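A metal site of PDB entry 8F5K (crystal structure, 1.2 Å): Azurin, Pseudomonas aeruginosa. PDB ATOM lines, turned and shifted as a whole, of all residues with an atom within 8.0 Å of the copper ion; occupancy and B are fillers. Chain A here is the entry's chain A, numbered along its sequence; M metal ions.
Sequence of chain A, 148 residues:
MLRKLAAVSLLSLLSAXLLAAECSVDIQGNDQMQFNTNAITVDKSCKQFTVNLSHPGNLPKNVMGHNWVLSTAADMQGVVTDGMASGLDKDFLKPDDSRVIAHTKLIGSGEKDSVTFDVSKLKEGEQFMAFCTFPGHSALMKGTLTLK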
ATOM      1  N   GLY A  29     -11.364   1.006   4.887  1.00  0.00           N
ATOM      2  CA  GLY A  29     -11.157   0.166   6.058  1.00  0.00           C
ATOM      3  C   GLY A  29     -12.406   0.261   6.913  1.00  0.00           C
ATOM      4  O   GLY A  29     -12.858   1.369   7.152  1.00  0.00           O
ATOM      5  N   ASN A  30     -12.958  -0.840   7.409  1.00  0.00           N
ATOM      6  CA  ASN A  30     -14.326  -0.793   7.955  1.00  0.00           C
ATOM      7  C   ASN A  30     -14.350  -1.322   9.389  1.00  0.00           C
ATOM      8  O   ASN A  30     -13.318  -1.543  10.009  1.00  0.00           O
ATOM      9  CB  ASN A  30     -15.290  -1.533   7.033  1.00  0.00           C
ATOM     10  CG  ASN A  30     -15.022  -2.997   6.985  1.00  0.00           C
ATOM     11  OD1 ASN A  30     -14.263  -3.529   7.790  1.00  0.00           O
ATOM     12  ND2 ASN A  30     -15.697  -3.668   6.076  1.00  0.00           N
ATOM     13  N   MET A  33     -12.772  -4.673  10.503  1.00  0.00           N
ATOM     14  CA  MET A  33     -11.321  -4.812  10.549  1.00  0.00           C
ATOM     15  C   MET A  33     -10.758  -5.412   9.262  1.00  0.00           C
ATOM     16  O   MET A  33      -9.871  -6.251   9.302  1.00  0.00           O
ATOM     17  CB  MET A  33     -10.876  -5.594  11.790  1.00  0.00           C
ATOM     18  CG  MET A  33      -9.488  -5.314  12.257  1.00  0.00           C
ATOM     19  SD  MET A  33      -9.003  -6.373  13.624  1.00  0.00           S
ATOM     20  CE  MET A  33      -8.745  -7.922  12.718  1.00  0.00           C
ATOM     21  N   GLN A  34     -11.343  -5.019   8.130  1.00  0.00           N
ATOM     22  CA  GLN A  34     -10.838  -5.399   6.816  1.00  0.00           C
ATOM     23  C   GLN A  34     -10.705  -4.175   5.921  1.00  0.00           C
ATOM     24  O   GLN A  34     -11.513  -3.247   5.994  1.00  0.00           O
ATOM     25  CB  GLN A  34     -11.786  -6.387   6.139  1.00  0.00           C
ATOM     26  CG  GLN A  34     -11.792  -7.769   6.759  1.00  0.00           C
ATOM     27  CD  GLN A  34     -12.696  -8.715   6.012  1.00  0.00           C
ATOM     28  OE1 GLN A  34     -13.887  -8.451   5.859  1.00  0.00           O
ATOM     29  NE2 GLN A  34     -12.139  -9.808   5.539  1.00  0.00           N
ATOM     30  N   PHE A  35      -9.689  -4.192   5.070  1.00  0.00           N
ATOM     31  CA  PHE A  35      -9.724  -3.342   3.905  1.00  0.00           C
ATOM     32  C   PHE A  35     -10.647  -3.981   2.857  1.00  0.00           C
ATOM     33  O   PHE A  35     -10.945  -5.169   2.916  1.00  0.00           O
ATOM     34  CB  PHE A  35      -8.354  -3.214   3.274  1.00  0.00           C
ATOM     35  CG  PHE A  35      -7.330  -2.439   4.087  1.00  0.00           C
ATOM     36  CD1 PHE A  35      -7.494  -1.089   4.388  1.00  0.00           C
ATOM     37  CD2 PHE A  35      -6.140  -3.037   4.443  1.00  0.00           C
ATOM     38  CE1 PHE A  35      -6.502  -0.421   5.072  1.00  0.00           C
ATOM     39  CE2 PHE A  35      -5.163  -2.365   5.115  1.00  0.00           C
ATOM     40  CZ  PHE A  35      -5.355  -1.058   5.418  1.00  0.00           C
ATOM     41  N   LEU A  53      -7.876   6.541   1.147  1.00  0.00           N
ATOM     42  CA  LEU A  53      -8.416   5.729   2.218  1.00  0.00           C
ATOM     43  C   LEU A  53      -9.618   6.432   2.833  1.00  0.00           C
ATOM     44  O   LEU A  53      -9.606   7.639   3.062  1.00  0.00           O
ATOM     45  CB  LEU A  53      -7.325   5.552   3.282  1.00  0.00           C
ATOM     46  CG  LEU A  53      -7.747   4.676   4.460  1.00  0.00           C
ATOM     47  CD1 LEU A  53      -7.943   3.231   4.029  1.00  0.00           C
ATOM     48  CD2 LEU A  53      -6.701   4.746   5.556  1.00  0.00           C
ATOM     49  N   HIS A  55     -13.119   5.471   5.776  1.00  0.00           N
ATOM     50  CA  HIS A  55     -13.567   4.630   6.870  1.00  0.00           C
ATOM     51  C   HIS A  55     -15.086   4.705   6.900  1.00  0.00           C
ATOM     52  O   HIS A  55     -15.673   5.613   7.521  1.00  0.00           O
ATOM     53  CB  HIS A  55     -12.947   5.090   8.188  1.00  0.00           C
ATOM     54  CG  HIS A  55     -13.103   4.122   9.300  1.00  0.00           C
ATOM     55  ND1 HIS A  55     -14.261   3.406   9.526  1.00  0.00           N
ATOM     56  CD2 HIS A  55     -12.255   3.769  10.290  1.00  0.00           C
ATOM     57  CE1 HIS A  55     -14.103   2.637  10.587  1.00  0.00           C
ATOM     58  NE2 HIS A  55     -12.903   2.847  11.079  1.00  0.00           N
ATOM     59  N   LYS A  61     -11.702   6.408  15.848  1.00  0.00           N
ATOM     60  CA  LYS A  61     -10.302   6.131  15.582  1.00  0.00           C
ATOM     61  C   LYS A  61      -9.615   5.414  16.748  1.00  0.00           C
ATOM     62  O   LYS A  61      -8.712   4.603  16.521  1.00  0.00           O
ATOM     63  CB  LYS A  61      -9.597   7.443  15.300  1.00  0.00           C
ATOM     64  CG  LYS A  61      -8.169   7.268  14.844  1.00  0.00           C
ATOM     65  CD  LYS A  61      -7.580   8.598  14.418  1.00  0.00           C
ATOM     66  CE  LYS A  61      -7.478   9.603  15.529  1.00  0.00           C
ATOM     67  NZ  LYS A  61      -6.958  10.924  15.054  1.00  0.00           N
ATOM     68  N   VAL A  63     -10.846   3.182  18.657  1.00  0.00           N
ATOM     69  CA  VAL A  63     -11.397   1.843  18.808  1.00  0.00           C
ATOM     70  C   VAL A  63     -11.072   0.989  17.589  1.00  0.00           C
ATOM     71  O   VAL A  63     -10.663  -0.171  17.720  1.00  0.00           O
ATOM     72  CB  VAL A  63     -12.922   1.884  19.059  1.00  0.00           C
ATOM     73  CG1 VAL A  63     -13.508   0.496  19.009  1.00  0.00           C
ATOM     74  CG2 VAL A  63     -13.240   2.516  20.383  1.00  0.00           C
ATOM     75  N   MET A  64     -11.283   1.539  16.399  1.00  0.00           N
ATOM     76  CA  MET A  64     -11.142   0.812  15.142  1.00  0.00           C
ATOM     77  C   MET A  64     -10.512   1.745  14.120  1.00  0.00           C
ATOM     78  O   MET A  64     -11.000   1.913  12.998  1.00  0.00           O
ATOM     79  CB  MET A  64     -12.506   0.302  14.724  1.00  0.00           C
ATOM     80  CG  MET A  64     -12.599  -0.480  13.473  1.00  0.00           C
ATOM     81  SD  MET A  64     -11.560  -2.002  13.389  1.00  0.00           S
ATOM     82  CE  MET A  64     -12.189  -3.080  14.679  1.00  0.00           C
ATOM     83  N   GLY A  65      -9.422   2.391  14.532  1.00  0.00           N
ATOM     84  CA  GLY A  65      -8.711   3.265  13.632  1.00  0.00           C
ATOM     85  C   GLY A  65      -7.966   2.494  12.563  1.00  0.00           C
ATOM     86  O   GLY A  65      -7.525   1.348  12.759  1.00  0.00           O
ATOM     87  N   HIS A  66      -7.842   3.097  11.389  1.00  0.00           N
ATOM     88  CA  HIS A  66      -7.117   2.459  10.312  1.00  0.00           C
ATOM     89  C   HIS A  66      -6.180   3.432   9.641  1.00  0.00           C
ATOM     90  O   HIS A  66      -6.523   4.596   9.430  1.00  0.00           O
ATOM     91  CB  HIS A  66      -8.088   1.984   9.236  1.00  0.00           C
ATOM     92  CG  HIS A  66      -9.083   0.971   9.704  1.00  0.00           C
ATOM     93  ND1 HIS A  66      -8.739  -0.159  10.411  1.00  0.00           N
ATOM     94  CD2 HIS A  66     -10.418   0.892   9.472  1.00  0.00           C
ATOM     95  CE1 HIS A  66      -9.829  -0.859  10.656  1.00  0.00           C
ATOM     96  NE2 HIS A  66     -10.863  -0.255  10.079  1.00  0.00           N
ATOM     97  N   ASN A  67      -5.027   2.934   9.256  1.00  0.00           N
ATOM     98  CA  ASN A  67      -4.146   3.616   8.338  1.00  0.00           C
ATOM     99  C   ASN A  67      -3.852   2.656   7.199  1.00  0.00           C
ATOM    100  O   ASN A  67      -4.270   1.498   7.206  1.00  0.00           O
ATOM    101  CB  ASN A  67      -2.860   4.124   8.979  1.00  0.00           C
ATOM    102  CG  ASN A  67      -2.113   3.096   9.782  1.00  0.00           C
ATOM    103  OD1 ASN A  67      -2.323   1.892   9.649  1.00  0.00           O
ATOM    104  ND2 ASN A  67      -1.198   3.556  10.596  1.00  0.00           N
ATOM    105  N   TRP A  68      -3.187   3.175   6.177  1.00  0.00           N
ATOM    106  CA  TRP A  68      -2.719   2.390   5.052  1.00  0.00           C
ATOM    107  C   TRP A  68      -1.221   2.632   4.952  1.00  0.00           C
ATOM    108  O   TRP A  68      -0.794   3.772   4.767  1.00  0.00           O
ATOM    109  CB  TRP A  68      -3.447   2.795   3.775  1.00  0.00           C
ATOM    110  CG  TRP A  68      -3.124   1.907   2.610  1.00  0.00           C
ATOM    111  CD1 TRP A  68      -3.763   0.785   2.253  1.00  0.00           C
ATOM    112  CD2 TRP A  68      -2.055   2.070   1.664  1.00  0.00           C
ATOM    113  NE1 TRP A  68      -3.191   0.226   1.132  1.00  0.00           N
ATOM    114  CE2 TRP A  68      -2.117   0.987   0.767  1.00  0.00           C
ATOM    115  CE3 TRP A  68      -1.046   3.010   1.507  1.00  0.00           C
ATOM    116  CZ2 TRP A  68      -1.240   0.828  -0.290  1.00  0.00           C
ATOM    117  CZ3 TRP A  68      -0.151   2.838   0.440  1.00  0.00           C
ATOM    118  CH2 TRP A  68      -0.249   1.753  -0.430  1.00  0.00           C
ATOM    119  N   LEU A 106      -3.765   7.859  10.445  1.00  0.00           N
ATOM    120  CA  LEU A 106      -4.770   7.012  11.066  1.00  0.00           C
ATOM    121  C   LEU A 106      -6.092   7.745  11.096  1.00  0.00           C
ATOM    122  O   LEU A 106      -6.135   8.923  11.429  1.00  0.00           O
ATOM    123  CB  LEU A 106      -4.323   6.655  12.492  1.00  0.00           C
ATOM    124  CG  LEU A 106      -5.111   5.551  13.176  1.00  0.00           C
ATOM    125  CD1 LEU A 106      -4.635   4.186  12.685  1.00  0.00           C
ATOM    126  CD2 LEU A 106      -4.954   5.675  14.692  1.00  0.00           C
ATOM    127  N   ILE A 107      -7.165   7.050  10.694  1.00  0.00           N
ATOM    128  CA  ILE A 107      -8.490   7.636  10.593  1.00  0.00           C
ATOM    129  C   ILE A 107      -9.518   6.755  11.279  1.00  0.00           C
ATOM    130  O   ILE A 107      -9.392   5.538  11.362  1.00  0.00           O
ATOM    131  CB  ILE A 107      -8.917   7.904   9.144  1.00  0.00           C
ATOM    132  CG1 ILE A 107      -8.976   6.621   8.315  1.00  0.00           C
ATOM    133  CG2 ILE A 107      -7.968   8.918   8.506  1.00  0.00           C
ATOM    134  CD1 ILE A 107      -9.674   6.788   6.931  1.00  0.00           C
ATOM    135  N   PHE A 131      -0.759  -2.545   4.711  1.00  0.00           N
ATOM    136  CA  PHE A 131      -1.320  -3.037   5.955  1.00  0.00           C
ATOM    137  C   PHE A 131      -1.731  -1.863   6.829  1.00  0.00           C
ATOM    138  O   PHE A 131      -1.383  -0.715   6.565  1.00  0.00           O
ATOM    139  CB  PHE A 131      -0.320  -3.958   6.698  1.00  0.00           C
ATOM    140  CG  PHE A 131       1.049  -3.365   6.834  1.00  0.00           C
ATOM    141  CD1 PHE A 131       1.966  -3.505   5.801  1.00  0.00           C
ATOM    142  CD2 PHE A 131       1.396  -2.642   7.965  1.00  0.00           C
ATOM    143  CE1 PHE A 131       3.213  -2.947   5.894  1.00  0.00           C
ATOM    144  CE2 PHE A 131       2.639  -2.097   8.076  1.00  0.00           C
ATOM    145  CZ  PHE A 131       3.571  -2.280   7.040  1.00  0.00           C
ATOM    146  N   CYS A 132      -2.491  -2.170   7.881  1.00  0.00           N
ATOM    147  CA  CYS A 132      -2.839  -1.219   8.938  1.00  0.00           C
ATOM    148  C   CYS A 132      -2.051  -1.562  10.197  1.00  0.00           C
ATOM    149  O   CYS A 132      -1.872  -2.751  10.501  1.00  0.00           O
ATOM    150  CB  CYS A 132      -4.334  -1.327   9.228  1.00  0.00           C
ATOM    151  SG  CYS A 132      -4.848  -0.278  10.585  1.00  0.00           S
ATOM    152  N   THR A 133      -1.565  -0.546  10.895  1.00  0.00           N
ATOM    153  CA  THR A 133      -0.756  -0.773  12.090  1.00  0.00           C
ATOM    154  C   THR A 133      -1.508  -0.594  13.405  1.00  0.00           C
ATOM    155  O   THR A 133      -0.887  -0.667  14.463  1.00  0.00           O
ATOM    156  CB  THR A 133       0.517   0.055  12.088  1.00  0.00           C
ATOM    157  OG1 THR A 133       0.136   1.438  12.148  1.00  0.00           O
ATOM    158  CG2 THR A 133       1.370  -0.205  10.880  1.00  0.00           C
ATOM    159  N   PHE A 134      -2.819  -0.329  13.380  1.00  0.00           N
ATOM    160  CA  PHE A 134      -3.560  -0.298  14.629  1.00  0.00           C
ATOM    161  C   PHE A 134      -3.471  -1.657  15.303  1.00  0.00           C
ATOM    162  O   PHE A 134      -3.557  -2.694  14.628  1.00  0.00           O
ATOM    163  CB  PHE A 134      -5.017   0.042  14.357  1.00  0.00           C
ATOM    164  CG  PHE A 134      -5.822   0.422  15.584  1.00  0.00           C
ATOM    165  CD1 PHE A 134      -6.355  -0.537  16.414  1.00  0.00           C
ATOM    166  CD2 PHE A 134      -6.033   1.751  15.884  1.00  0.00           C
ATOM    167  CE1 PHE A 134      -7.116  -0.146  17.527  1.00  0.00           C
ATOM    168  CE2 PHE A 134      -6.794   2.111  16.987  1.00  0.00           C
ATOM    169  CZ  PHE A 134      -7.327   1.189  17.798  1.00  0.00           C
ATOM    170  N   PRO A 135      -3.293  -1.713  16.615  1.00  0.00           N
ATOM    171  CA  PRO A 135      -3.002  -3.000  17.247  1.00  0.00           C
ATOM    172  C   PRO A 135      -3.987  -4.096  16.899  1.00  0.00           C
ATOM    173  O   PRO A 135      -5.204  -3.959  17.070  1.00  0.00           O
ATOM    174  CB  PRO A 135      -3.035  -2.650  18.737  1.00  0.00           C
ATOM    175  CG  PRO A 135      -2.518  -1.241  18.748  1.00  0.00           C
ATOM    176  CD  PRO A 135      -3.112  -0.579  17.532  1.00  0.00           C
ATOM    177  N   GLY A 136      -3.433  -5.210  16.438  1.00  0.00           N
ATOM    178  CA  GLY A 136      -4.163  -6.385  16.057  1.00  0.00           C
ATOM    179  C   GLY A 136      -4.653  -6.409  14.628  1.00  0.00           C
ATOM    180  O   GLY A 136      -4.910  -7.510  14.088  1.00  0.00           O
ATOM    181  N   HIS A 137      -4.767  -5.249  13.992  1.00  0.00           N
ATOM    182  CA  HIS A 137      -5.550  -5.211  12.762  1.00  0.00           C
ATOM    183  C   HIS A 137      -4.910  -5.994  11.638  1.00  0.00           C
ATOM    184  O   HIS A 137      -5.621  -6.495  10.770  1.00  0.00           O
ATOM    185  CB  HIS A 137      -5.782  -3.780  12.304  1.00  0.00           C
ATOM    186  CG  HIS A 137      -6.814  -3.089  13.111  1.00  0.00           C
ATOM    187  ND1 HIS A 137      -7.384  -1.886  12.722  1.00  0.00           N
ATOM    188  CD2 HIS A 137      -7.368  -3.398  14.316  1.00  0.00           C
ATOM    189  CE1 HIS A 137      -8.246  -1.507  13.646  1.00  0.00           C
ATOM    190  NE2 HIS A 137      -8.261  -2.401  14.615  1.00  0.00           N
ATOM    191  N   SER A 138      -3.575  -6.053  11.595  1.00  0.00           N
ATOM    192  CA  SER A 138      -2.919  -6.700  10.469  1.00  0.00           C
ATOM    193  C   SER A 138      -3.136  -8.196  10.416  1.00  0.00           C
ATOM    194  O   SER A 138      -2.724  -8.801   9.424  1.00  0.00           O
ATOM    195  CB  SER A 138      -1.427  -6.370  10.457  1.00  0.00           C
ATOM    196  OG  SER A 138      -0.768  -7.007  11.524  1.00  0.00           O
ATOM    197  N   MET A 141      -5.856  -7.060   8.061  1.00  0.00           N
ATOM    198  CA  MET A 141      -5.612  -5.862   7.264  1.00  0.00           C
ATOM    199  C   MET A 141      -4.176  -5.893   6.754  1.00  0.00           C
ATOM    200  O   MET A 141      -3.305  -5.135   7.197  1.00  0.00           O
ATOM    201  CB  MET A 141      -5.940  -4.622   8.062  1.00  0.00           C
ATOM    202  CG  MET A 141      -7.404  -4.618   8.451  1.00  0.00           C
ATOM    203  SD  MET A 141      -7.940  -3.107   9.261  1.00  0.00           S
ATOM    204  CE  MET A 141      -8.099  -2.040   7.825  1.00  0.00           C
HETATM  205 CU    CU M   1      -6.929  -0.732  11.137  1.00  0.00          CU
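N of Phe 134 lies close to SG of Cys 132 (3.5 Å).
A ring nitrogen (ND1) of His 137 sits close to the backbone carbonyl oxygen (O) of Gly 65, 3.2 Å away.
ND1 of His 66 sits close to SD of Met 141 (3.3 Å).
The side-chain sulfur (SG) of Cys 132 sits close to the side-chain amide oxygen (OD1) of Asn 67 (3.5 Å).
A ring nitrogen (ND1) of His 137 lies close to the side-chain sulfur of Met 141 (3.7 Å).
The backbone NH of Ile 107 lies within hydrogen-bond range of the backbone carbonyl oxygen of His 66, 2.8 Å away.
O of Asn 30 lies within hydrogen-bond range of NE2 of His 66 (2.8 Å).
A ring nitrogen (NE2) of His 137 sits close to the side-chain sulfur (SD) of Met 64, 3.5 Å away.
Merely in contact with the copper ion: Phe 134 and Met 141.
Within 4 Å of the copper ion: Gly 65, His 66, Cys 132, Phe 134, His 137 and Met 141.
A ring nitrogen (ND1) of His 137 binds the copper ion (2.0 Å).
The copper ion is bound by ND1 of His 66 (2.0 Å).
The copper ion is bound by SG of Cys 132 (2.2 Å).
The copper ion has three donor atoms within binding distance.
Slightly farther from the copper ion lies the backbone carbonyl oxygen (O) of Gly 65 (2.7 Å).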
